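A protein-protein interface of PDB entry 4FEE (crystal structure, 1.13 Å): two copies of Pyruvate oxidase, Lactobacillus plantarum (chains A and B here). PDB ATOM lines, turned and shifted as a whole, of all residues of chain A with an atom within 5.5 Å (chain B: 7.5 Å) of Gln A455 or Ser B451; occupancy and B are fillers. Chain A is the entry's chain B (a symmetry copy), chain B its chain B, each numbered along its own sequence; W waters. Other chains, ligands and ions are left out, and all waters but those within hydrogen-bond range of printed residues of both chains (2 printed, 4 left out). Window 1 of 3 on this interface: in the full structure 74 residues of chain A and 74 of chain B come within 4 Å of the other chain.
Of the 24 printed residues of chain B, 10 touch a printed residue of chain A. Hydrophobic or aromatic side chains of chain B that line the printed part of chain A: His B58, Met B452, Met B454, Tyr B477, Phe B497 and Ile B500. Along chain B the printed residues that touch a printed residue of chain A span positions 58 to 500. Among the printed residues, 12 pairs touch across the chains. Among the printed residues, no Asp or Glu carboxylate lies within 4 Å of a Lys or Arg side-chain nitrogen of the other chain.
His A58 touches Met B452, and with the chains exchanged Met A452 touches His B58. Ser A451 touches Gln B455, and with the chains exchanged Gln A455 touches Ser B451. Met A454 touches its own counterpart, Met B454. Of the 12 pairs that touch across the chains among the printed residues, 5 have their exchanged pair printed and touching as well.
NE2 of His A58 lies within hydrogen-bond range of OE2 of Glu B60 (2.8 Å). O of Asn B498 is in hydrogen-bond range of NH2 of Arg A57 (2.9 Å). The side-chain sulfur of Met A454 sits close to the side-chain sulfur of Met B454 (3.3 Å).
Of the printed residues of chain B, Gln A455 touches Ser B451 (3.4 Å). Of the printed residues of chain A, Ser B451 touches Gln A455 (3.4 Å). Printed residues of chain A within 4 Å of Ile B500: Arg A57 and Ala A458. Of the printed residues of chain A, Met B454 touches Met A454 (3.3 Å). Gly B423 touches none of the printed residues of chain A. The nearest printed residue of chain B that does not touch Gln A455 is Met B454 (4.02 Å).
The backbone NH of Glu B60 lies close to a ring nitrogen (ND1) of His B58. The backbone carbonyl oxygen of Asp B447 sits at hydrogen-bond distance from the side-chain hydroxyl of Ser B451 (2.7 Å). OD1 of Asp A456 is in hydrogen-bond range of N of Arg A57, at 2.8 Å. The backbone NH (N) of His A58 sits at hydrogen-bond distance from the side-chain carboxylate (OD2) of Asp A456, 3.2 Å away. The side-chain amide nitrogen of Gln A455 sits at hydrogen-bond distance from the side-chain carboxylate of Asp A456, at 2.9 Å.
Water W2 lies within hydrogen-bond range of O of Arg A57 (2.7 Å), OH of Tyr B477 (2.8 Å) and O of Gly B448 (3.0 Å). Water W1 lies within hydrogen-bond range of OE2 of Glu B60 (3.3 Å), NE2 of His B58 (3.3 Å) and NE2 of His A58 (3.3 Å).
Met B452 touches Arg A57. Arg A57 touches Tyr B477. Phe B497 touches Arg A57 (CD1 to NH1, 3.6 Å). Arg A57 touches Ile B500 (NH1 to CD1, 3.7 Å). His A58 touches Met B452 (CD2 to O, 3.7 Å). Ser A451 touches Gln B455 (O to CB, 3.4 Å). His B58 touches Met A452 (CD2 to O, 3.7 Å). CB of Gln A455 touches O of Ser B451, 3.4 Å away. CD1 of Ile B500 touches CB of Ala A458, at 3.9 Å.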
ATOM      1  N   ARG A  57      -1.053  27.012 -15.092  1.00  0.00           N
ATOM      2  CA  ARG A  57      -1.732  26.696 -13.834  1.00  0.00           C
ATOM      3  C   ARG A  57      -3.201  27.093 -13.861  1.00  0.00           C
ATOM      4  O   ARG A  57      -3.944  26.658 -12.947  1.00  0.00           O
ATOM      5  CB  ARG A  57      -1.020  27.289 -12.631  1.00  0.00           C
ATOM      6  CG  ARG A  57       0.433  26.881 -12.474  1.00  0.00           C
ATOM      7  CD  ARG A  57       0.806  25.472 -12.664  1.00  0.00           C
ATOM      8  NE  ARG A  57       2.252  25.132 -12.364  1.00  0.00           N
ATOM      9  CZ  ARG A  57       2.753  24.891 -11.176  1.00  0.00           C
ATOM     10  NH1 ARG A  57       2.039  24.751 -10.035  1.00  0.00           N
ATOM     11  NH2 ARG A  57       4.098  24.725 -11.128  1.00  0.00           N
ATOM     12  N   HIS A  58      -3.643  27.856 -14.832  1.00  0.00           N
ATOM     13  CA  HIS A  58      -5.033  28.184 -15.043  1.00  0.00           C
ATOM     14  C   HIS A  58      -5.225  28.343 -16.539  1.00  0.00           C
ATOM     15  O   HIS A  58      -4.423  29.033 -17.202  1.00  0.00           O
ATOM     16  CB  HIS A  58      -5.410  29.458 -14.289  1.00  0.00           C
ATOM     17  CG  HIS A  58      -6.848  29.819 -14.257  1.00  0.00           C
ATOM     18  ND1 HIS A  58      -7.575  30.080 -15.318  1.00  0.00           N
ATOM     19  CD2 HIS A  58      -7.672  30.059 -13.205  1.00  0.00           C
ATOM     20  CE1 HIS A  58      -8.810  30.429 -15.032  1.00  0.00           C
ATOM     21  NE2 HIS A  58      -8.904  30.433 -13.690  1.00  0.00           N
ATOM     22  N   VAL A  61      -4.796  31.610 -18.590  1.00  0.00           N
ATOM     23  CA  VAL A  61      -3.458  32.077 -18.884  1.00  0.00           C
ATOM     24  C   VAL A  61      -2.976  31.461 -20.200  1.00  0.00           C
ATOM     25  O   VAL A  61      -2.283  32.136 -20.978  1.00  0.00           O
ATOM     26  CB  VAL A  61      -2.531  31.789 -17.703  1.00  0.00           C
ATOM     27  CG1 VAL A  61      -1.045  31.950 -18.060  1.00  0.00           C
ATOM     28  CG2 VAL A  61      -2.925  32.671 -16.529  1.00  0.00           C
ATOM     29  N   SER A 451      -3.073  39.936  -9.369  1.00  0.00           N
ATOM     30  CA  SER A 451      -3.800  39.016  -8.500  1.00  0.00           C
ATOM     31  C   SER A 451      -4.571  38.002  -9.323  1.00  0.00           C
ATOM     32  O   SER A 451      -4.626  36.827  -8.938  1.00  0.00           O
ATOM     33  CB  SER A 451      -4.727  39.785  -7.573  1.00  0.00           C
ATOM     34  OG  SER A 451      -4.048  40.526  -6.578  1.00  0.00           O
ATOM     35  N   MET A 452      -5.163  38.408 -10.301  1.00  0.00           N
ATOM     36  CA  MET A 452      -6.045  37.490 -11.033  1.00  0.00           C
ATOM     37  C   MET A 452      -5.284  36.332 -11.671  1.00  0.00           C
ATOM     38  O   MET A 452      -5.842  35.229 -11.764  1.00  0.00           O
ATOM     39  CB  MET A 452      -6.886  38.213 -12.073  1.00  0.00           C
ATOM     40  CG  MET A 452      -7.985  39.064 -11.486  1.00  0.00           C
ATOM     41  SD  MET A 452      -8.798  40.043 -12.752  1.00  0.00           S
ATOM     42  CE  MET A 452     -10.163  40.711 -11.838  1.00  0.00           C
ATOM     43  N   THR A 453      -4.050  36.549 -12.117  1.00  0.00           N
ATOM     44  CA  THR A 453      -3.277  35.503 -12.781  1.00  0.00           C
ATOM     45  C   THR A 453      -2.013  35.129 -12.030  1.00  0.00           C
ATOM     46  O   THR A 453      -1.096  34.484 -12.570  1.00  0.00           O
ATOM     47  CB  THR A 453      -3.033  35.814 -14.259  1.00  0.00           C
ATOM     48  OG1 THR A 453      -2.428  37.117 -14.357  1.00  0.00           O
ATOM     49  CG2 THR A 453      -4.315  35.754 -15.064  1.00  0.00           C
ATOM     50  N   MET A 454      -1.943  35.449 -10.722  1.00  0.00           N
ATOM     51  CA  MET A 454      -0.710  35.325  -9.970  1.00  0.00           C
ATOM     52  C   MET A 454      -0.149  33.922  -9.952  1.00  0.00           C
ATOM     53  O   MET A 454       1.078  33.742  -9.860  1.00  0.00           O
ATOM     54  CB  MET A 454      -0.896  35.774  -8.479  1.00  0.00           C
ATOM     55  CG  MET A 454      -1.878  34.908  -7.671  1.00  0.00           C
ATOM     56  SD  MET A 454      -1.913  35.022  -5.846  1.00  0.00           S
ATOM     57  CE  MET A 454      -1.973  36.752  -5.783  1.00  0.00           C
ATOM     58  N   GLN A 455      -1.013  32.894  -9.980  1.00  0.00           N
ATOM     59  CA  GLN A 455      -0.491  31.543  -9.893  1.00  0.00           C
ATOM     60  C   GLN A 455       0.431  31.207 -11.022  1.00  0.00           C
ATOM     61  O   GLN A 455       1.318  30.342 -10.871  1.00  0.00           O
ATOM     62  CB  GLN A 455      -1.662  30.530  -9.849  1.00  0.00           C
ATOM     63  CG  GLN A 455      -2.416  30.388 -11.149  1.00  0.00           C
ATOM     64  CD  GLN A 455      -3.280  31.555 -11.552  1.00  0.00           C
ATOM     65  OE1 GLN A 455      -3.788  32.324 -10.720  1.00  0.00           O
ATOM     66  NE2 GLN A 455      -3.442  31.696 -12.866  1.00  0.00           N
ATOM     67  N   ASP A 456       0.265  31.861 -12.186  1.00  0.00           N
ATOM     68  CA  ASP A 456       1.127  31.568 -13.331  1.00  0.00           C
ATOM     69  C   ASP A 456       2.481  32.269 -13.310  1.00  0.00           C
ATOM     70  O   ASP A 456       3.317  32.059 -14.179  1.00  0.00           O
ATOM     71  CB  ASP A 456       0.361  31.729 -14.652  1.00  0.00           C
ATOM     72  CG  ASP A 456      -0.403  30.442 -14.939  1.00  0.00           C
ATOM     73  OD1 ASP A 456       0.195  29.509 -15.523  1.00  0.00           O
ATOM     74  OD2 ASP A 456      -1.598  30.318 -14.592  1.00  0.00           O
ATOM     75  N   LEU A 457       2.768  33.007 -12.217  1.00  0.00           N
ATOM     76  CA  LEU A 457       4.179  33.262 -11.904  1.00  0.00           C
ATOM     77  C   LEU A 457       4.945  31.942 -11.813  1.00  0.00           C
ATOM     78  O   LEU A 457       6.118  31.859 -12.159  1.00  0.00           O
ATOM     79  CB  LEU A 457       4.297  34.078 -10.633  1.00  0.00           C
ATOM     80  CG  LEU A 457       3.790  35.510 -10.715  1.00  0.00           C
ATOM     81  CD1 LEU A 457       3.701  36.137  -9.317  1.00  0.00           C
ATOM     82  CD2 LEU A 457       4.632  36.403 -11.604  1.00  0.00           C
ATOM     83  N   ALA A 458       4.275  30.874 -11.312  1.00  0.00           N
ATOM     84  CA  ALA A 458       4.953  29.580 -11.206  1.00  0.00           C
ATOM     85  C   ALA A 458       5.329  29.038 -12.567  1.00  0.00           C
ATOM     86  O   ALA A 458       6.302  28.280 -12.667  1.00  0.00           O
ATOM     87  CB  ALA A 458       4.065  28.594 -10.485  1.00  0.00           C
ATOM     88  N   THR A 459       4.587  29.398 -13.627  1.00  0.00           N
ATOM     89  CA  THR A 459       4.942  28.951 -14.964  1.00  0.00           C
ATOM     90  C   THR A 459       6.216  29.590 -15.467  1.00  0.00           C
ATOM     91  O   THR A 459       7.012  28.961 -16.163  1.00  0.00           O
ATOM     92  CB  THR A 459       3.730  29.256 -15.886  1.00  0.00           C
ATOM     93  OG1 THR A 459       2.597  28.630 -15.280  1.00  0.00           O
ATOM     94  CG2 THR A 459       3.938  28.780 -17.298  1.00  0.00           C
ATOM     95  N   VAL A 509       6.180  30.768  -5.081  1.00  0.00           N
ATOM     96  CA  VAL A 509       6.371  30.039  -6.341  1.00  0.00           C
ATOM     97  C   VAL A 509       7.840  29.857  -6.679  1.00  0.00           C
ATOM     98  O   VAL A 509       8.192  29.349  -7.769  1.00  0.00           O
ATOM     99  CB  VAL A 509       5.599  30.686  -7.500  1.00  0.00           C
ATOM    100  CG1 VAL A 509       4.104  30.850  -7.204  1.00  0.00           C
ATOM    101  CG2 VAL A 509       6.175  32.039  -7.925  1.00  0.00           C
ATOM    102  N   HIS B  58     -11.196  37.711  -8.013  1.00  0.00           N
ATOM    103  CA  HIS B  58     -11.422  37.217  -9.350  1.00  0.00           C
ATOM    104  C   HIS B  58     -12.898  36.885  -9.452  1.00  0.00           C
ATOM    105  O   HIS B  58     -13.453  36.221  -8.553  1.00  0.00           O
ATOM    106  CB  HIS B  58     -10.550  35.994  -9.630  1.00  0.00           C
ATOM    107  CG  HIS B  58     -10.532  35.486 -11.024  1.00  0.00           C
ATOM    108  ND1 HIS B  58     -11.586  35.040 -11.667  1.00  0.00           N
ATOM    109  CD2 HIS B  58      -9.492  35.268 -11.867  1.00  0.00           C
ATOM    110  CE1 HIS B  58     -11.310  34.592 -12.873  1.00  0.00           C
ATOM    111  NE2 HIS B  58      -9.980  34.717 -13.030  1.00  0.00           N
ATOM    112  N   GLU B  60     -14.724  34.781 -11.002  1.00  0.00           N
ATOM    113  CA  GLU B  60     -15.072  33.374 -10.980  1.00  0.00           C
ATOM    114  C   GLU B  60     -15.331  32.943  -9.547  1.00  0.00           C
ATOM    115  O   GLU B  60     -16.205  32.108  -9.304  1.00  0.00           O
ATOM    116  CB  GLU B  60     -14.057  32.432 -11.619  1.00  0.00           C
ATOM    117  CG  GLU B  60     -12.903  31.938 -10.848  1.00  0.00           C
ATOM    118  CD  GLU B  60     -12.068  30.985 -11.673  1.00  0.00           C
ATOM    119  OE1 GLU B  60     -12.599  29.857 -11.976  1.00  0.00           O
ATOM    120  OE2 GLU B  60     -10.925  31.340 -12.002  1.00  0.00           O
ATOM    121  N   ASP B 393     -12.608  20.773  -3.044  1.00  0.00           N
ATOM    122  CA  ASP B 393     -12.225  21.062  -4.426  1.00  0.00           C
ATOM    123  C   ASP B 393     -12.371  19.782  -5.279  1.00  0.00           C
ATOM    124  O   ASP B 393     -13.095  18.867  -4.880  1.00  0.00           O
ATOM    125  CB  ASP B 393     -10.834  21.717  -4.467  1.00  0.00           C
ATOM    126  CG  ASP B 393     -10.636  22.736  -5.591  1.00  0.00           C
ATOM    127  OD1 ASP B 393     -10.562  22.337  -6.774  1.00  0.00           O
ATOM    128  OD2 ASP B 393     -10.598  23.960  -5.281  1.00  0.00           O
ATOM    129  N   MET B 422     -12.496  22.645 -11.011  1.00  0.00           N
ATOM    130  CA  MET B 422     -11.475  22.947 -10.033  1.00  0.00           C
ATOM    131  C   MET B 422     -11.595  24.397  -9.560  1.00  0.00           C
ATOM    132  O   MET B 422     -12.096  25.272 -10.271  1.00  0.00           O
ATOM    133  CB  MET B 422     -10.110  22.719 -10.604  1.00  0.00           C
ATOM    134  CG  MET B 422      -9.772  21.275 -10.869  1.00  0.00           C
ATOM    135  SD  MET B 422      -8.341  21.101 -11.942  1.00  0.00           S
ATOM    136  CE  MET B 422      -7.031  21.747 -10.917  1.00  0.00           C
ATOM    137  N   GLY B 423     -11.102  24.643  -8.353  1.00  0.00           N
ATOM    138  CA  GLY B 423     -11.019  25.946  -7.772  1.00  0.00           C
ATOM    139  C   GLY B 423     -12.113  26.273  -6.810  1.00  0.00           C
ATOM    140  O   GLY B 423     -12.068  27.311  -6.145  1.00  0.00           O
ATOM    141  N   ILE B 426     -11.942  27.192  -2.212  1.00  0.00           N
ATOM    142  CA  ILE B 426     -11.886  28.511  -1.591  1.00  0.00           C
ATOM    143  C   ILE B 426     -13.227  29.219  -1.611  1.00  0.00           C
ATOM    144  O   ILE B 426     -13.677  29.650  -0.545  1.00  0.00           O
ATOM    145  CB  ILE B 426     -10.714  29.316  -2.198  1.00  0.00           C
ATOM    146  CG1 ILE B 426      -9.367  28.749  -1.729  1.00  0.00           C
ATOM    147  CG2 ILE B 426     -10.860  30.812  -1.902  1.00  0.00           C
ATOM    148  CD1 ILE B 426      -8.156  29.237  -2.520  1.00  0.00           C
ATOM    149  N   ALA B 445      -8.503  21.044  -0.471  1.00  0.00           N
ATOM    150  CA  ALA B 445      -8.209  21.252  -1.896  1.00  0.00           C
ATOM    151  C   ALA B 445      -6.874  20.652  -2.247  1.00  0.00           C
ATOM    152  O   ALA B 445      -5.905  20.724  -1.481  1.00  0.00           O
ATOM    153  CB  ALA B 445      -8.166  22.763  -2.181  1.00  0.00           C
ATOM    154  N   GLY B 446      -6.803  20.102  -3.451  1.00  0.00           N
ATOM    155  CA  GLY B 446      -5.512  19.783  -4.043  1.00  0.00           C
ATOM    156  C   GLY B 446      -4.728  21.041  -4.426  1.00  0.00           C
ATOM    157  O   GLY B 446      -5.289  22.114  -4.543  1.00  0.00           O
ATOM    158  N   ASP B 447      -3.445  20.871  -4.660  1.00  0.00           N
ATOM    159  CA  ASP B 447      -2.579  21.990  -5.054  1.00  0.00           C
ATOM    160  C   ASP B 447      -2.979  22.566  -6.387  1.00  0.00           C
ATOM    161  O   ASP B 447      -2.938  23.799  -6.580  1.00  0.00           O
ATOM    162  CB  ASP B 447      -1.120  21.619  -5.001  1.00  0.00           C
ATOM    163  CG  ASP B 447      -0.619  20.386  -5.696  1.00  0.00           C
ATOM    164  OD1 ASP B 447      -1.433  19.603  -6.258  1.00  0.00           O
ATOM    165  OD2 ASP B 447       0.605  20.145  -5.594  1.00  0.00           O
ATOM    166  N   GLY B 448      -3.388  21.744  -7.366  1.00  0.00           N
ATOM    167  CA  GLY B 448      -3.830  22.256  -8.630  1.00  0.00           C
ATOM    168  C   GLY B 448      -5.048  23.168  -8.532  1.00  0.00           C
ATOM    169  O   GLY B 448      -5.100  24.262  -9.102  1.00  0.00           O
ATOM    170  N   GLY B 449      -6.055  22.708  -7.770  1.00  0.00           N
ATOM    171  CA  GLY B 449      -7.291  23.471  -7.610  1.00  0.00           C
ATOM    172  C   GLY B 449      -7.116  24.686  -6.735  1.00  0.00           C
ATOM    173  O   GLY B 449      -7.628  25.768  -7.059  1.00  0.00           O
ATOM    174  N   ALA B 450      -6.353  24.556  -5.642  1.00  0.00           N
ATOM    175  CA  ALA B 450      -6.090  25.690  -4.807  1.00  0.00           C
ATOM    176  C   ALA B 450      -5.358  26.780  -5.590  1.00  0.00           C
ATOM    177  O   ALA B 450      -5.585  27.972  -5.383  1.00  0.00           O
ATOM    178  CB  ALA B 450      -5.291  25.276  -3.585  1.00  0.00           C
ATOM    179  N   SER B 451      -4.452  26.389  -6.468  1.00  0.00           N
ATOM    180  CA  SER B 451      -3.713  27.310  -7.326  1.00  0.00           C
ATOM    181  C   SER B 451      -4.668  28.145  -8.157  1.00  0.00           C
ATOM    182  O   SER B 451      -4.414  29.341  -8.351  1.00  0.00           O
ATOM    183  CB  SER B 451      -2.744  26.545  -8.213  1.00  0.00           C
ATOM    184  OG  SER B 451      -1.651  25.987  -7.510  1.00  0.00           O
ATOM    185  N   MET B 452      -5.618  27.579  -8.656  1.00  0.00           N
ATOM    186  CA  MET B 452      -6.477  28.317  -9.591  1.00  0.00           C
ATOM    187  C   MET B 452      -7.206  29.479  -8.924  1.00  0.00           C
ATOM    188  O   MET B 452      -7.438  30.500  -9.588  1.00  0.00           O
ATOM    189  CB  MET B 452      -7.464  27.405 -10.303  1.00  0.00           C
ATOM    190  CG  MET B 452      -6.830  26.506 -11.335  1.00  0.00           C
ATOM    191  SD  MET B 452      -8.012  25.321 -11.982  1.00  0.00           S
ATOM    192  CE  MET B 452      -7.083  24.608 -13.313  1.00  0.00           C
ATOM    193  N   THR B 453      -7.581  29.350  -7.655  1.00  0.00           N
ATOM    194  CA  THR B 453      -8.324  30.400  -6.962  1.00  0.00           C
ATOM    195  C   THR B 453      -7.571  30.982  -5.780  1.00  0.00           C
ATOM    196  O   THR B 453      -8.144  31.663  -4.910  1.00  0.00           O
ATOM    197  CB  THR B 453      -9.751  29.966  -6.617  1.00  0.00           C
ATOM    198  OG1 THR B 453      -9.686  28.732  -5.877  1.00  0.00           O
ATOM    199  CG2 THR B 453     -10.604  29.805  -7.858  1.00  0.00           C
ATOM    200  N   MET B 454      -6.235  30.808  -5.741  1.00  0.00           N
ATOM    201  CA  MET B 454      -5.456  31.140  -4.565  1.00  0.00           C
ATOM    202  C   MET B 454      -5.568  32.590  -4.153  1.00  0.00           C
ATOM    203  O   MET B 454      -5.450  32.908  -2.957  1.00  0.00           O
ATOM    204  CB  MET B 454      -3.933  30.829  -4.775  1.00  0.00           C
ATOM    205  CG  MET B 454      -3.259  31.663  -5.878  1.00  0.00           C
ATOM    206  SD  MET B 454      -1.435  31.735  -5.990  1.00  0.00           S
ATOM    207  CE  MET B 454      -1.190  30.024  -5.874  1.00  0.00           C
ATOM    208  N   GLN B 455      -5.737  33.511  -5.115  1.00  0.00           N
ATOM    209  CA  GLN B 455      -5.777  34.912  -4.740  1.00  0.00           C
ATOM    210  C   GLN B 455      -6.901  35.226  -3.804  1.00  0.00           C
ATOM    211  O   GLN B 455      -6.810  36.192  -3.019  1.00  0.00           O
ATOM    212  CB  GLN B 455      -5.885  35.792  -6.010  1.00  0.00           C
ATOM    213  CG  GLN B 455      -7.220  35.718  -6.711  1.00  0.00           C
ATOM    214  CD  GLN B 455      -7.527  34.430  -7.429  1.00  0.00           C
ATOM    215  OE1 GLN B 455      -6.637  33.701  -7.896  1.00  0.00           O
ATOM    216  NE2 GLN B 455      -8.823  34.138  -7.513  1.00  0.00           N
ATOM    217  N   VAL B 471      -4.377  22.292   2.046  1.00  0.00           N
ATOM    218  CA  VAL B 471      -3.925  22.058   0.682  1.00  0.00           C
ATOM    219  C   VAL B 471      -3.127  20.780   0.645  1.00  0.00           C
ATOM    220  O   VAL B 471      -2.219  20.594   1.432  1.00  0.00           O
ATOM    221  CB  VAL B 471      -3.126  23.256   0.135  1.00  0.00           C
ATOM    222  CG1 VAL B 471      -2.663  22.962  -1.292  1.00  0.00           C
ATOM    223  CG2 VAL B 471      -3.908  24.563   0.212  1.00  0.00           C
ATOM    224  N   TYR B 477      -1.191  16.950 -10.898  1.00  0.00           N
ATOM    225  CA  TYR B 477      -2.642  16.737 -11.124  1.00  0.00           C
ATOM    226  C   TYR B 477      -2.853  15.244 -10.951  1.00  0.00           C
ATOM    227  O   TYR B 477      -2.891  14.485 -11.928  1.00  0.00           O
ATOM    228  CB  TYR B 477      -3.056  17.222 -12.486  1.00  0.00           C
ATOM    229  CG  TYR B 477      -2.880  18.691 -12.748  1.00  0.00           C
ATOM    230  CD1 TYR B 477      -3.435  19.668 -11.906  1.00  0.00           C
ATOM    231  CD2 TYR B 477      -2.204  19.147 -13.832  1.00  0.00           C
ATOM    232  CE1 TYR B 477      -3.281  21.003 -12.164  1.00  0.00           C
ATOM    233  CE2 TYR B 477      -2.044  20.495 -14.077  1.00  0.00           C
ATOM    234  CZ  TYR B 477      -2.586  21.433 -13.236  1.00  0.00           C
ATOM    235  OH  TYR B 477      -2.395  22.767 -13.499  1.00  0.00           O
ATOM    236  N   PHE B 497       4.461  18.837 -11.816  1.00  0.00           N
ATOM    237  CA  PHE B 497       4.837  20.243 -11.954  1.00  0.00           C
ATOM    238  C   PHE B 497       5.606  20.669 -10.705  1.00  0.00           C
ATOM    239  O   PHE B 497       5.782  19.957  -9.747  1.00  0.00           O
ATOM    240  CB  PHE B 497       3.619  21.109 -12.254  1.00  0.00           C
ATOM    241  CG  PHE B 497       2.413  20.870 -11.375  1.00  0.00           C
ATOM    242  CD1 PHE B 497       2.422  21.201 -10.035  1.00  0.00           C
ATOM    243  CD2 PHE B 497       1.256  20.338 -11.908  1.00  0.00           C
ATOM    244  CE1 PHE B 497       1.325  21.016  -9.226  1.00  0.00           C
ATOM    245  CE2 PHE B 497       0.157  20.152 -11.103  1.00  0.00           C
ATOM    246  CZ  PHE B 497       0.187  20.515  -9.796  1.00  0.00           C
ATOM    247  N   ASN B 498       6.107  21.908 -10.766  1.00  0.00           N
ATOM    248  CA  ASN B 498       6.911  22.489  -9.722  1.00  0.00           C
ATOM    249  C   ASN B 498       6.091  22.957  -8.518  1.00  0.00           C
ATOM    250  O   ASN B 498       5.020  23.538  -8.677  1.00  0.00           O
ATOM    251  CB  ASN B 498       7.682  23.727 -10.237  1.00  0.00           C
ATOM    252  CG  ASN B 498       8.847  23.375 -11.108  1.00  0.00           C
ATOM    253  OD1 ASN B 498       9.088  22.241 -11.496  1.00  0.00           O
ATOM    254  ND2 ASN B 498       9.660  24.404 -11.358  1.00  0.00           N
ATOM    255  N   ILE B 500       4.526  24.763  -5.349  1.00  0.00           N
ATOM    256  CA  ILE B 500       4.163  26.041  -4.790  1.00  0.00           C
ATOM    257  C   ILE B 500       4.045  25.877  -3.286  1.00  0.00           C
ATOM    258  O   ILE B 500       3.374  24.949  -2.806  1.00  0.00           O
ATOM    259  CB  ILE B 500       2.840  26.602  -5.364  1.00  0.00           C
ATOM    260  CG1 ILE B 500       2.983  26.878  -6.843  1.00  0.00           C
ATOM    261  CG2 ILE B 500       2.382  27.817  -4.561  1.00  0.00           C
ATOM    262  CD1 ILE B 500       1.737  27.417  -7.520  1.00  0.00           C
ATOM    263  N   PHE B 502       2.296  26.911  -0.336  1.00  0.00           N
ATOM    264  CA  PHE B 502       1.075  27.629   0.007  1.00  0.00           C
ATOM    265  C   PHE B 502       1.170  28.265   1.396  1.00  0.00           C
ATOM    266  O   PHE B 502       0.374  29.170   1.669  1.00  0.00           O
ATOM    267  CB  PHE B 502      -0.163  26.728  -0.096  1.00  0.00           C
ATOM    268  CG  PHE B 502      -0.744  26.706  -1.475  1.00  0.00           C
ATOM    269  CD1 PHE B 502      -1.734  27.593  -1.795  1.00  0.00           C
ATOM    270  CD2 PHE B 502      -0.287  25.770  -2.389  1.00  0.00           C
ATOM    271  CE1 PHE B 502      -2.296  27.585  -3.087  1.00  0.00           C
ATOM    272  CE2 PHE B 502      -0.789  25.789  -3.677  1.00  0.00           C
ATOM    273  CZ  PHE B 502      -1.779  26.707  -4.008  1.00  0.00           C
ATOM    274  N   ILE B 505       2.327  31.579   0.142  1.00  0.00           N
ATOM    275  CA  ILE B 505       1.213  32.254  -0.461  1.00  0.00           C
ATOM    276  C   ILE B 505       0.296  32.832   0.617  1.00  0.00           C
ATOM    277  O   ILE B 505      -0.096  34.015   0.554  1.00  0.00           O
ATOM    278  CB  ILE B 505       0.420  31.302  -1.369  1.00  0.00           C
ATOM    279  CG1 ILE B 505       1.262  30.699  -2.499  1.00  0.00           C
ATOM    280  CG2 ILE B 505      -0.838  31.975  -1.923  1.00  0.00           C
ATOM    281  CD1 ILE B 505       1.864  31.709  -3.458  1.00  0.00           C
HETATM  282  O   HOH W   1     -11.227  32.390 -15.071  1.00  0.00           O
HETATM  283  O   HOH W   2      -3.365  24.440 -11.509  1.00  0.00           O
